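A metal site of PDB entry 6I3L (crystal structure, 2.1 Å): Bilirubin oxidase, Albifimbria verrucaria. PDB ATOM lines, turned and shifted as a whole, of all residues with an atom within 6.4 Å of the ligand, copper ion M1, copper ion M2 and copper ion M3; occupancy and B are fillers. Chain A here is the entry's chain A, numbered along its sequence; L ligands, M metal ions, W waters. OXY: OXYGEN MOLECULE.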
ATOM      1  N   HIS A  94     -24.188 -21.697 -25.475  1.00  0.00           N
ATOM      2  CA  HIS A  94     -24.294 -23.018 -26.128  1.00  0.00           C
ATOM      3  C   HIS A  94     -24.742 -24.064 -25.111  1.00  0.00           C
ATOM      4  O   HIS A  94     -24.037 -24.209 -24.077  1.00  0.00           O
ATOM      5  CB  HIS A  94     -22.938 -23.404 -26.727  1.00  0.00           C
ATOM      6  CG  HIS A  94     -22.915 -24.795 -27.223  1.00  0.00           C
ATOM      7  ND1 HIS A  94     -23.839 -25.243 -28.139  1.00  0.00           N
ATOM      8  CD2 HIS A  94     -22.056 -25.814 -26.976  1.00  0.00           C
ATOM      9  CE1 HIS A  94     -23.552 -26.493 -28.449  1.00  0.00           C
ATOM     10  NE2 HIS A  94     -22.465 -26.858 -27.730  1.00  0.00           N
ATOM     11  N   LEU A  95     -25.826 -24.788 -25.420  1.00  0.00           N
ATOM     12  CA  LEU A  95     -26.242 -26.036 -24.739  1.00  0.00           C
ATOM     13  C   LEU A  95     -25.512 -27.215 -25.395  1.00  0.00           C
ATOM     14  O   LEU A  95     -25.939 -27.705 -26.474  1.00  0.00           O
ATOM     15  CB  LEU A  95     -27.767 -26.223 -24.811  1.00  0.00           C
ATOM     16  CG  LEU A  95     -28.329 -27.402 -24.023  1.00  0.00           C
ATOM     17  CD1 LEU A  95     -27.827 -27.365 -22.588  1.00  0.00           C
ATOM     18  CD2 LEU A  95     -29.854 -27.404 -24.038  1.00  0.00           C
ATOM     19  N   HIS A  96     -24.425 -27.619 -24.781  1.00  0.00           N
ATOM     20  CA  HIS A  96     -23.526 -28.688 -25.296  1.00  0.00           C
ATOM     21  C   HIS A  96     -24.209 -30.049 -25.063  1.00  0.00           C
ATOM     22  O   HIS A  96     -24.479 -30.407 -23.898  1.00  0.00           O
ATOM     23  CB  HIS A  96     -22.168 -28.513 -24.612  1.00  0.00           C
ATOM     24  CG  HIS A  96     -21.097 -29.384 -25.167  1.00  0.00           C
ATOM     25  ND1 HIS A  96     -19.833 -28.924 -25.395  1.00  0.00           N
ATOM     26  CD2 HIS A  96     -21.113 -30.682 -25.554  1.00  0.00           C
ATOM     27  CE1 HIS A  96     -19.094 -29.901 -25.868  1.00  0.00           C
ATOM     28  NE2 HIS A  96     -19.852 -30.982 -25.985  1.00  0.00           N
ATOM     29  N   GLY A  97     -24.514 -30.764 -26.135  1.00  0.00           N
ATOM     30  CA  GLY A  97     -25.175 -32.084 -26.096  1.00  0.00           C
ATOM     31  C   GLY A  97     -26.566 -32.029 -26.706  1.00  0.00           C
ATOM     32  O   GLY A  97     -27.193 -33.093 -26.743  1.00  0.00           O
ATOM     33  N   ASP A 105     -27.995 -22.339 -30.902  1.00  0.00           N
ATOM     34  CA  ASP A 105     -26.890 -23.291 -30.588  1.00  0.00           C
ATOM     35  C   ASP A 105     -25.653 -22.578 -30.020  1.00  0.00           C
ATOM     36  O   ASP A 105     -24.725 -23.307 -29.645  1.00  0.00           O
ATOM     37  CB  ASP A 105     -26.428 -24.065 -31.821  1.00  0.00           C
ATOM     38  CG  ASP A 105     -25.603 -25.303 -31.505  1.00  0.00           C
ATOM     39  OD1 ASP A 105     -26.012 -26.071 -30.586  1.00  0.00           O
ATOM     40  OD2 ASP A 105     -24.544 -25.494 -32.176  1.00  0.00           O
ATOM     41  N   GLY A 106     -25.621 -21.247 -29.934  1.00  0.00           N
ATOM     42  CA  GLY A 106     -24.462 -20.483 -29.433  1.00  0.00           C
ATOM     43  C   GLY A 106     -23.353 -20.328 -30.476  1.00  0.00           C
ATOM     44  O   GLY A 106     -22.157 -20.278 -30.083  1.00  0.00           O
ATOM     45  N   TRP A 132     -24.384 -29.626 -20.717  1.00  0.00           N
ATOM     46  CA  TRP A 132     -23.944 -28.454 -19.964  1.00  0.00           C
ATOM     47  C   TRP A 132     -24.103 -27.247 -20.877  1.00  0.00           C
ATOM     48  O   TRP A 132     -24.064 -27.420 -22.099  1.00  0.00           O
ATOM     49  CB  TRP A 132     -22.547 -28.695 -19.364  1.00  0.00           C
ATOM     50  CG  TRP A 132     -21.402 -28.817 -20.335  1.00  0.00           C
ATOM     51  CD1 TRP A 132     -21.243 -29.724 -21.344  1.00  0.00           C
ATOM     52  CD2 TRP A 132     -20.217 -28.018 -20.319  1.00  0.00           C
ATOM     53  NE1 TRP A 132     -20.057 -29.505 -21.981  1.00  0.00           N
ATOM     54  CE2 TRP A 132     -19.398 -28.462 -21.375  1.00  0.00           C
ATOM     55  CE3 TRP A 132     -19.774 -26.967 -19.518  1.00  0.00           C
ATOM     56  CZ2 TRP A 132     -18.153 -27.903 -21.638  1.00  0.00           C
ATOM     57  CZ3 TRP A 132     -18.554 -26.393 -19.783  1.00  0.00           C
ATOM     58  CH2 TRP A 132     -17.760 -26.858 -20.835  1.00  0.00           C
ATOM     59  N   HIS A 134     -22.889 -23.209 -21.588  1.00  0.00           N
ATOM     60  CA  HIS A 134     -21.673 -22.409 -21.318  1.00  0.00           C
ATOM     61  C   HIS A 134     -21.464 -21.360 -22.393  1.00  0.00           C
ATOM     62  O   HIS A 134     -22.100 -21.441 -23.476  1.00  0.00           O
ATOM     63  CB  HIS A 134     -20.432 -23.300 -21.173  1.00  0.00           C
ATOM     64  CG  HIS A 134     -20.036 -24.029 -22.404  1.00  0.00           C
ATOM     65  ND1 HIS A 134     -19.417 -23.405 -23.461  1.00  0.00           N
ATOM     66  CD2 HIS A 134     -20.115 -25.324 -22.725  1.00  0.00           C
ATOM     67  CE1 HIS A 134     -19.119 -24.300 -24.388  1.00  0.00           C
ATOM     68  NE2 HIS A 134     -19.545 -25.474 -23.968  1.00  0.00           N
ATOM     69  N   ASP A 135     -20.551 -20.439 -22.104  1.00  0.00           N
ATOM     70  CA  ASP A 135     -20.334 -19.309 -23.017  1.00  0.00           C
ATOM     71  C   ASP A 135     -19.578 -19.806 -24.227  1.00  0.00           C
ATOM     72  O   ASP A 135     -18.791 -20.751 -24.092  1.00  0.00           O
ATOM     73  CB  ASP A 135     -19.614 -18.135 -22.351  1.00  0.00           C
ATOM     74  CG  ASP A 135     -19.681 -16.958 -23.301  1.00  0.00           C
ATOM     75  OD1 ASP A 135     -20.844 -16.545 -23.588  1.00  0.00           O
ATOM     76  OD2 ASP A 135     -18.619 -16.595 -23.839  1.00  0.00           O
ATOM     77  N   HIS A 136     -19.865 -19.205 -25.383  1.00  0.00           N
ATOM     78  CA  HIS A 136     -19.258 -19.577 -26.683  1.00  0.00           C
ATOM     79  C   HIS A 136     -18.922 -18.307 -27.483  1.00  0.00           C
ATOM     80  O   HIS A 136     -18.673 -18.434 -28.666  1.00  0.00           O
ATOM     81  CB  HIS A 136     -20.194 -20.537 -27.412  1.00  0.00           C
ATOM     82  CG  HIS A 136     -19.492 -21.561 -28.241  1.00  0.00           C
ATOM     83  ND1 HIS A 136     -18.495 -21.216 -29.142  1.00  0.00           N
ATOM     84  CD2 HIS A 136     -19.637 -22.901 -28.312  1.00  0.00           C
ATOM     85  CE1 HIS A 136     -18.036 -22.308 -29.732  1.00  0.00           C
ATOM     86  NE2 HIS A 136     -18.719 -23.372 -29.238  1.00  0.00           N
ATOM     87  N   ALA A 274     -14.804 -30.850 -21.876  1.00  0.00           N
ATOM     88  CA  ALA A 274     -16.189 -30.887 -22.409  1.00  0.00           C
ATOM     89  C   ALA A 274     -16.723 -32.315 -22.408  1.00  0.00           C
ATOM     90  O   ALA A 274     -17.902 -32.483 -22.645  1.00  0.00           O
ATOM     91  CB  ALA A 274     -16.287 -30.242 -23.770  1.00  0.00           C
ATOM     92  N   HIS A 401     -14.720 -31.453 -30.660  1.00  0.00           N
ATOM     93  CA  HIS A 401     -16.181 -31.427 -30.452  1.00  0.00           C
ATOM     94  C   HIS A 401     -16.835 -31.072 -31.768  1.00  0.00           C
ATOM     95  O   HIS A 401     -16.343 -30.141 -32.421  1.00  0.00           O
ATOM     96  CB  HIS A 401     -16.518 -30.381 -29.410  1.00  0.00           C
ATOM     97  CG  HIS A 401     -17.976 -30.201 -29.233  1.00  0.00           C
ATOM     98  ND1 HIS A 401     -18.848 -31.267 -29.188  1.00  0.00           N
ATOM     99  CD2 HIS A 401     -18.700 -29.059 -29.069  1.00  0.00           C
ATOM    100  CE1 HIS A 401     -20.066 -30.819 -28.974  1.00  0.00           C
ATOM    101  NE2 HIS A 401     -19.991 -29.457 -28.900  1.00  0.00           N
ATOM    102  N   ILE A 402     -17.892 -31.796 -32.116  1.00  0.00           N
ATOM    103  CA  ILE A 402     -18.737 -31.501 -33.299  1.00  0.00           C
ATOM    104  C   ILE A 402     -20.147 -31.184 -32.803  1.00  0.00           C
ATOM    105  O   ILE A 402     -20.778 -32.057 -32.164  1.00  0.00           O
ATOM    106  CB  ILE A 402     -18.720 -32.662 -34.303  1.00  0.00           C
ATOM    107  CG1 ILE A 402     -17.294 -33.117 -34.632  1.00  0.00           C
ATOM    108  CG2 ILE A 402     -19.494 -32.243 -35.560  1.00  0.00           C
ATOM    109  CD1 ILE A 402     -17.199 -34.375 -35.490  1.00  0.00           C
ATOM    110  N   HIS A 403     -20.639 -29.975 -33.111  1.00  0.00           N
ATOM    111  CA  HIS A 403     -22.036 -29.569 -32.786  1.00  0.00           C
ATOM    112  C   HIS A 403     -23.029 -30.422 -33.580  1.00  0.00           C
ATOM    113  O   HIS A 403     -22.615 -31.142 -34.492  1.00  0.00           O
ATOM    114  CB  HIS A 403     -22.271 -28.081 -33.043  1.00  0.00           C
ATOM    115  CG  HIS A 403     -21.571 -27.215 -32.065  1.00  0.00           C
ATOM    116  ND1 HIS A 403     -22.209 -26.227 -31.378  1.00  0.00           N
ATOM    117  CD2 HIS A 403     -20.266 -27.162 -31.682  1.00  0.00           C
ATOM    118  CE1 HIS A 403     -21.358 -25.612 -30.598  1.00  0.00           C
ATOM    119  NE2 HIS A 403     -20.146 -26.160 -30.762  1.00  0.00           N
ATOM    120  N   LEU A 404     -24.297 -30.319 -33.210  1.00  0.00           N
ATOM    121  CA  LEU A 404     -25.484 -30.988 -33.786  1.00  0.00           C
ATOM    122  C   LEU A 404     -25.490 -32.491 -33.442  1.00  0.00           C
ATOM    123  O   LEU A 404     -26.518 -32.953 -32.918  1.00  0.00           O
ATOM    124  CB  LEU A 404     -25.522 -30.774 -35.297  1.00  0.00           C
ATOM    125  CG  LEU A 404     -26.586 -31.615 -36.015  1.00  0.00           C
ATOM    126  CD1 LEU A 404     -27.976 -31.175 -35.561  1.00  0.00           C
ATOM    127  CD2 LEU A 404     -26.463 -31.525 -37.530  1.00  0.00           C
ATOM    128  N   ASP A 430     -19.847 -36.723 -28.172  1.00  0.00           N
ATOM    129  CA  ASP A 430     -19.803 -35.497 -29.009  1.00  0.00           C
ATOM    130  C   ASP A 430     -18.463 -34.763 -28.844  1.00  0.00           C
ATOM    131  O   ASP A 430     -18.270 -33.751 -29.536  1.00  0.00           O
ATOM    132  CB  ASP A 430     -21.003 -34.598 -28.726  1.00  0.00           C
ATOM    133  CG  ASP A 430     -21.144 -34.130 -27.290  1.00  0.00           C
ATOM    134  OD1 ASP A 430     -20.097 -33.928 -26.616  1.00  0.00           O
ATOM    135  OD2 ASP A 430     -22.316 -33.958 -26.881  1.00  0.00           O
ATOM    136  N   VAL A 431     -17.590 -35.242 -27.971  1.00  0.00           N
ATOM    137  CA  VAL A 431     -16.185 -34.809 -27.806  1.00  0.00           C
ATOM    138  C   VAL A 431     -15.320 -36.066 -27.850  1.00  0.00           C
ATOM    139  O   VAL A 431     -15.704 -37.079 -27.235  1.00  0.00           O
ATOM    140  CB  VAL A 431     -15.961 -34.067 -26.473  1.00  0.00           C
ATOM    141  CG1 VAL A 431     -14.541 -33.534 -26.326  1.00  0.00           C
ATOM    142  CG2 VAL A 431     -16.967 -32.958 -26.273  1.00  0.00           C
ATOM    143  N   MET A 454     -20.800 -25.342 -35.708  1.00  0.00           N
ATOM    144  CA  MET A 454     -19.361 -25.279 -35.424  1.00  0.00           C
ATOM    145  C   MET A 454     -18.817 -26.675 -35.123  1.00  0.00           C
ATOM    146  O   MET A 454     -19.571 -27.573 -34.788  1.00  0.00           O
ATOM    147  CB  MET A 454     -19.082 -24.337 -34.255  1.00  0.00           C
ATOM    148  CG  MET A 454     -19.464 -22.887 -34.557  1.00  0.00           C
ATOM    149  SD  MET A 454     -19.298 -21.809 -33.094  1.00  0.00           S
ATOM    150  CE  MET A 454     -20.401 -22.593 -31.924  1.00  0.00           C
ATOM    151  N   PHE A 455     -17.513 -26.846 -35.343  1.00  0.00           N
ATOM    152  CA  PHE A 455     -16.713 -27.950 -34.794  1.00  0.00           C
ATOM    153  C   PHE A 455     -15.323 -27.381 -34.490  1.00  0.00           C
ATOM    154  O   PHE A 455     -14.936 -26.379 -35.078  1.00  0.00           O
ATOM    155  CB  PHE A 455     -16.698 -29.175 -35.710  1.00  0.00           C
ATOM    156  CG  PHE A 455     -15.869 -29.074 -36.968  1.00  0.00           C
ATOM    157  CD1 PHE A 455     -16.343 -28.386 -38.075  1.00  0.00           C
ATOM    158  CD2 PHE A 455     -14.646 -29.686 -37.046  1.00  0.00           C
ATOM    159  CE1 PHE A 455     -15.601 -28.335 -39.246  1.00  0.00           C
ATOM    160  CE2 PHE A 455     -13.915 -29.655 -38.217  1.00  0.00           C
ATOM    161  CZ  PHE A 455     -14.391 -28.986 -39.315  1.00  0.00           C
ATOM    162  N   HIS A 456     -14.665 -27.921 -33.491  1.00  0.00           N
ATOM    163  CA  HIS A 456     -13.477 -27.251 -32.915  1.00  0.00           C
ATOM    164  C   HIS A 456     -12.842 -28.127 -31.848  1.00  0.00           C
ATOM    165  O   HIS A 456     -13.472 -29.096 -31.320  1.00  0.00           O
ATOM    166  CB  HIS A 456     -13.855 -25.889 -32.326  1.00  0.00           C
ATOM    167  CG  HIS A 456     -14.925 -25.942 -31.294  1.00  0.00           C
ATOM    168  ND1 HIS A 456     -14.659 -25.999 -29.938  1.00  0.00           N
ATOM    169  CD2 HIS A 456     -16.278 -25.950 -31.418  1.00  0.00           C
ATOM    170  CE1 HIS A 456     -15.793 -26.029 -29.267  1.00  0.00           C
ATOM    171  NE2 HIS A 456     -16.805 -25.999 -30.164  1.00  0.00           N
ATOM    172  N   HIS A 458     -11.899 -28.168 -27.960  1.00  0.00           N
ATOM    173  CA  HIS A 458     -12.505 -27.631 -26.719  1.00  0.00           C
ATOM    174  C   HIS A 458     -11.474 -27.308 -25.649  1.00  0.00           C
ATOM    175  O   HIS A 458     -11.921 -26.967 -24.488  1.00  0.00           O
ATOM    176  CB  HIS A 458     -13.568 -28.594 -26.168  1.00  0.00           C
ATOM    177  CG  HIS A 458     -14.781 -27.903 -25.622  1.00  0.00           C
ATOM    178  ND1 HIS A 458     -14.741 -27.199 -24.439  1.00  0.00           N
ATOM    179  CD2 HIS A 458     -16.067 -27.874 -26.049  1.00  0.00           C
ATOM    180  CE1 HIS A 458     -15.946 -26.721 -24.185  1.00  0.00           C
ATOM    181  NE2 HIS A 458     -16.789 -27.140 -25.142  1.00  0.00           N
ATOM    182  N   LEU A 460     -10.055 -24.354 -24.544  1.00  0.00           N
ATOM    183  CA  LEU A 460     -10.701 -23.053 -24.868  1.00  0.00           C
ATOM    184  C   LEU A 460      -9.627 -22.058 -25.335  1.00  0.00           C
ATOM    185  O   LEU A 460      -9.973 -21.134 -26.096  1.00  0.00           O
ATOM    186  CB  LEU A 460     -11.523 -22.553 -23.681  1.00  0.00           C
ATOM    187  CG  LEU A 460     -12.668 -23.479 -23.246  1.00  0.00           C
ATOM    188  CD1 LEU A 460     -13.383 -22.912 -22.033  1.00  0.00           C
ATOM    189  CD2 LEU A 460     -13.665 -23.734 -24.367  1.00  0.00           C
ATOM    190  N   GLU A 463      -9.297 -23.005 -29.046  1.00  0.00           N
ATOM    191  CA  GLU A 463     -10.572 -22.587 -29.688  1.00  0.00           C
ATOM    192  C   GLU A 463     -10.563 -21.065 -29.951  1.00  0.00           C
ATOM    193  O   GLU A 463     -10.964 -20.661 -31.046  1.00  0.00           O
ATOM    194  CB  GLU A 463     -11.736 -22.972 -28.769  1.00  0.00           C
ATOM    195  CG  GLU A 463     -13.104 -22.722 -29.367  1.00  0.00           C
ATOM    196  CD  GLU A 463     -14.234 -22.980 -28.382  1.00  0.00           C
ATOM    197  OE1 GLU A 463     -14.089 -23.934 -27.557  1.00  0.00           O
ATOM    198  OE2 GLU A 463     -15.243 -22.234 -28.444  1.00  0.00           O
ATOM    199  N   MET A 468     -11.198 -23.647 -34.858  1.00  0.00           N
ATOM    200  CA  MET A 468     -12.662 -23.781 -34.977  1.00  0.00           C
ATOM    201  C   MET A 468     -13.026 -23.494 -36.417  1.00  0.00           C
ATOM    202  O   MET A 468     -12.350 -22.700 -37.048  1.00  0.00           O
ATOM    203  CB  MET A 468     -13.355 -22.798 -34.029  1.00  0.00           C
ATOM    204  CG  MET A 468     -14.875 -22.902 -34.006  1.00  0.00           C
ATOM    205  SD  MET A 468     -15.467 -22.279 -32.415  1.00  0.00           S
ATOM    206  CE  MET A 468     -15.169 -20.522 -32.622  1.00  0.00           C
HETATM  207  O1  OXY L   1     -18.483 -25.871 -27.026  1.00  0.00           O
HETATM  208  O2  OXY L   1     -19.345 -26.573 -27.761  1.00  0.00           O
HETATM  209 CU    CU M   1     -18.692 -25.365 -29.564  1.00  0.00          CU
HETATM  210 CU    CU M   2     -19.013 -27.151 -25.031  1.00  0.00          CU
HETATM  211 CU    CU M   3     -21.225 -28.151 -28.302  1.00  0.00          CU
HETATM  212  O   HOH W   1     -23.647 -30.004 -28.955  1.00  0.00           O
HETATM  213  O   HOH W   2     -16.604 -24.095 -26.560  1.00  0.00           O
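Within 4 Å of copper ion M3: His 94, His 96, His 401 and His 403. The nearest printed residue that does not touch copper ion M3 is Gly 97 (4.7 Å).
The backbone NH of His 94 lies within hydrogen-bond range of the backbone carbonyl oxygen of His 134 (2.9 Å). The backbone carbonyl oxygen of Asp 105 sits at hydrogen-bond distance from a ring nitrogen (ND1) of His 94 (2.6 Å). A ring nitrogen (ND1) of His 401 sits close to a ring nitrogen (NE2) of His 96, 3.4 Å away. O of His 456 lies within hydrogen-bond range of N of His 401. ND1 of His 401 lies within hydrogen-bond range of O of Asp 430. A ring nitrogen (NE2) of His 96 sits at hydrogen-bond distance from the side-chain carboxylate (OD1) of Asp 430 (3.0 Å). The backbone NH of His 403 sits at hydrogen-bond distance from the backbone carbonyl oxygen of Met 454, 3.1 Å away. The side-chain carboxylate (OE1) of Glu 463 sits close to a ring nitrogen (ND1) of His 456, at 3.2 Å.
Hydrophobic or aromatic side chains within 4 Å of the ligand: His 94, His 96, His 134, His 136, His 401, His 403, His 456 and His 458. Along chain A the residues within 4 Å of the ligand span positions 94 to 458.
Copper ion M1 is bound by a ring nitrogen (NE2) of His 136 (2.0 Å), a ring nitrogen (NE2) of His 403 (2.0 Å), a ring nitrogen (NE2) of His 456 (2.1 Å) and an oxygen (O2) of the ligand (2.3 Å). Copper ion M1 has four donor atoms within binding distance.
Merely in contact with copper ion M2: Trp 132.
A ring nitrogen (NE2) of His 94 is bound to copper ion M3 (1.9 Å). A ring nitrogen (NE2) of His 401 is bound to copper ion M3. O2 of the ligand binds copper ion M3, 2.5 Å away.
Copper ion M2 is bound by ND1 of His 96 (2.0 Å), NE2 of His 134 (2.1 Å), NE2 of His 458 (2.2 Å) and O1 of the ligand (2.4 Å). Copper ion M2 has four donor atoms within binding distance.
Four residues have an atom within 4 Å of copper ion M1: His 136, His 401, His 403 and His 456.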
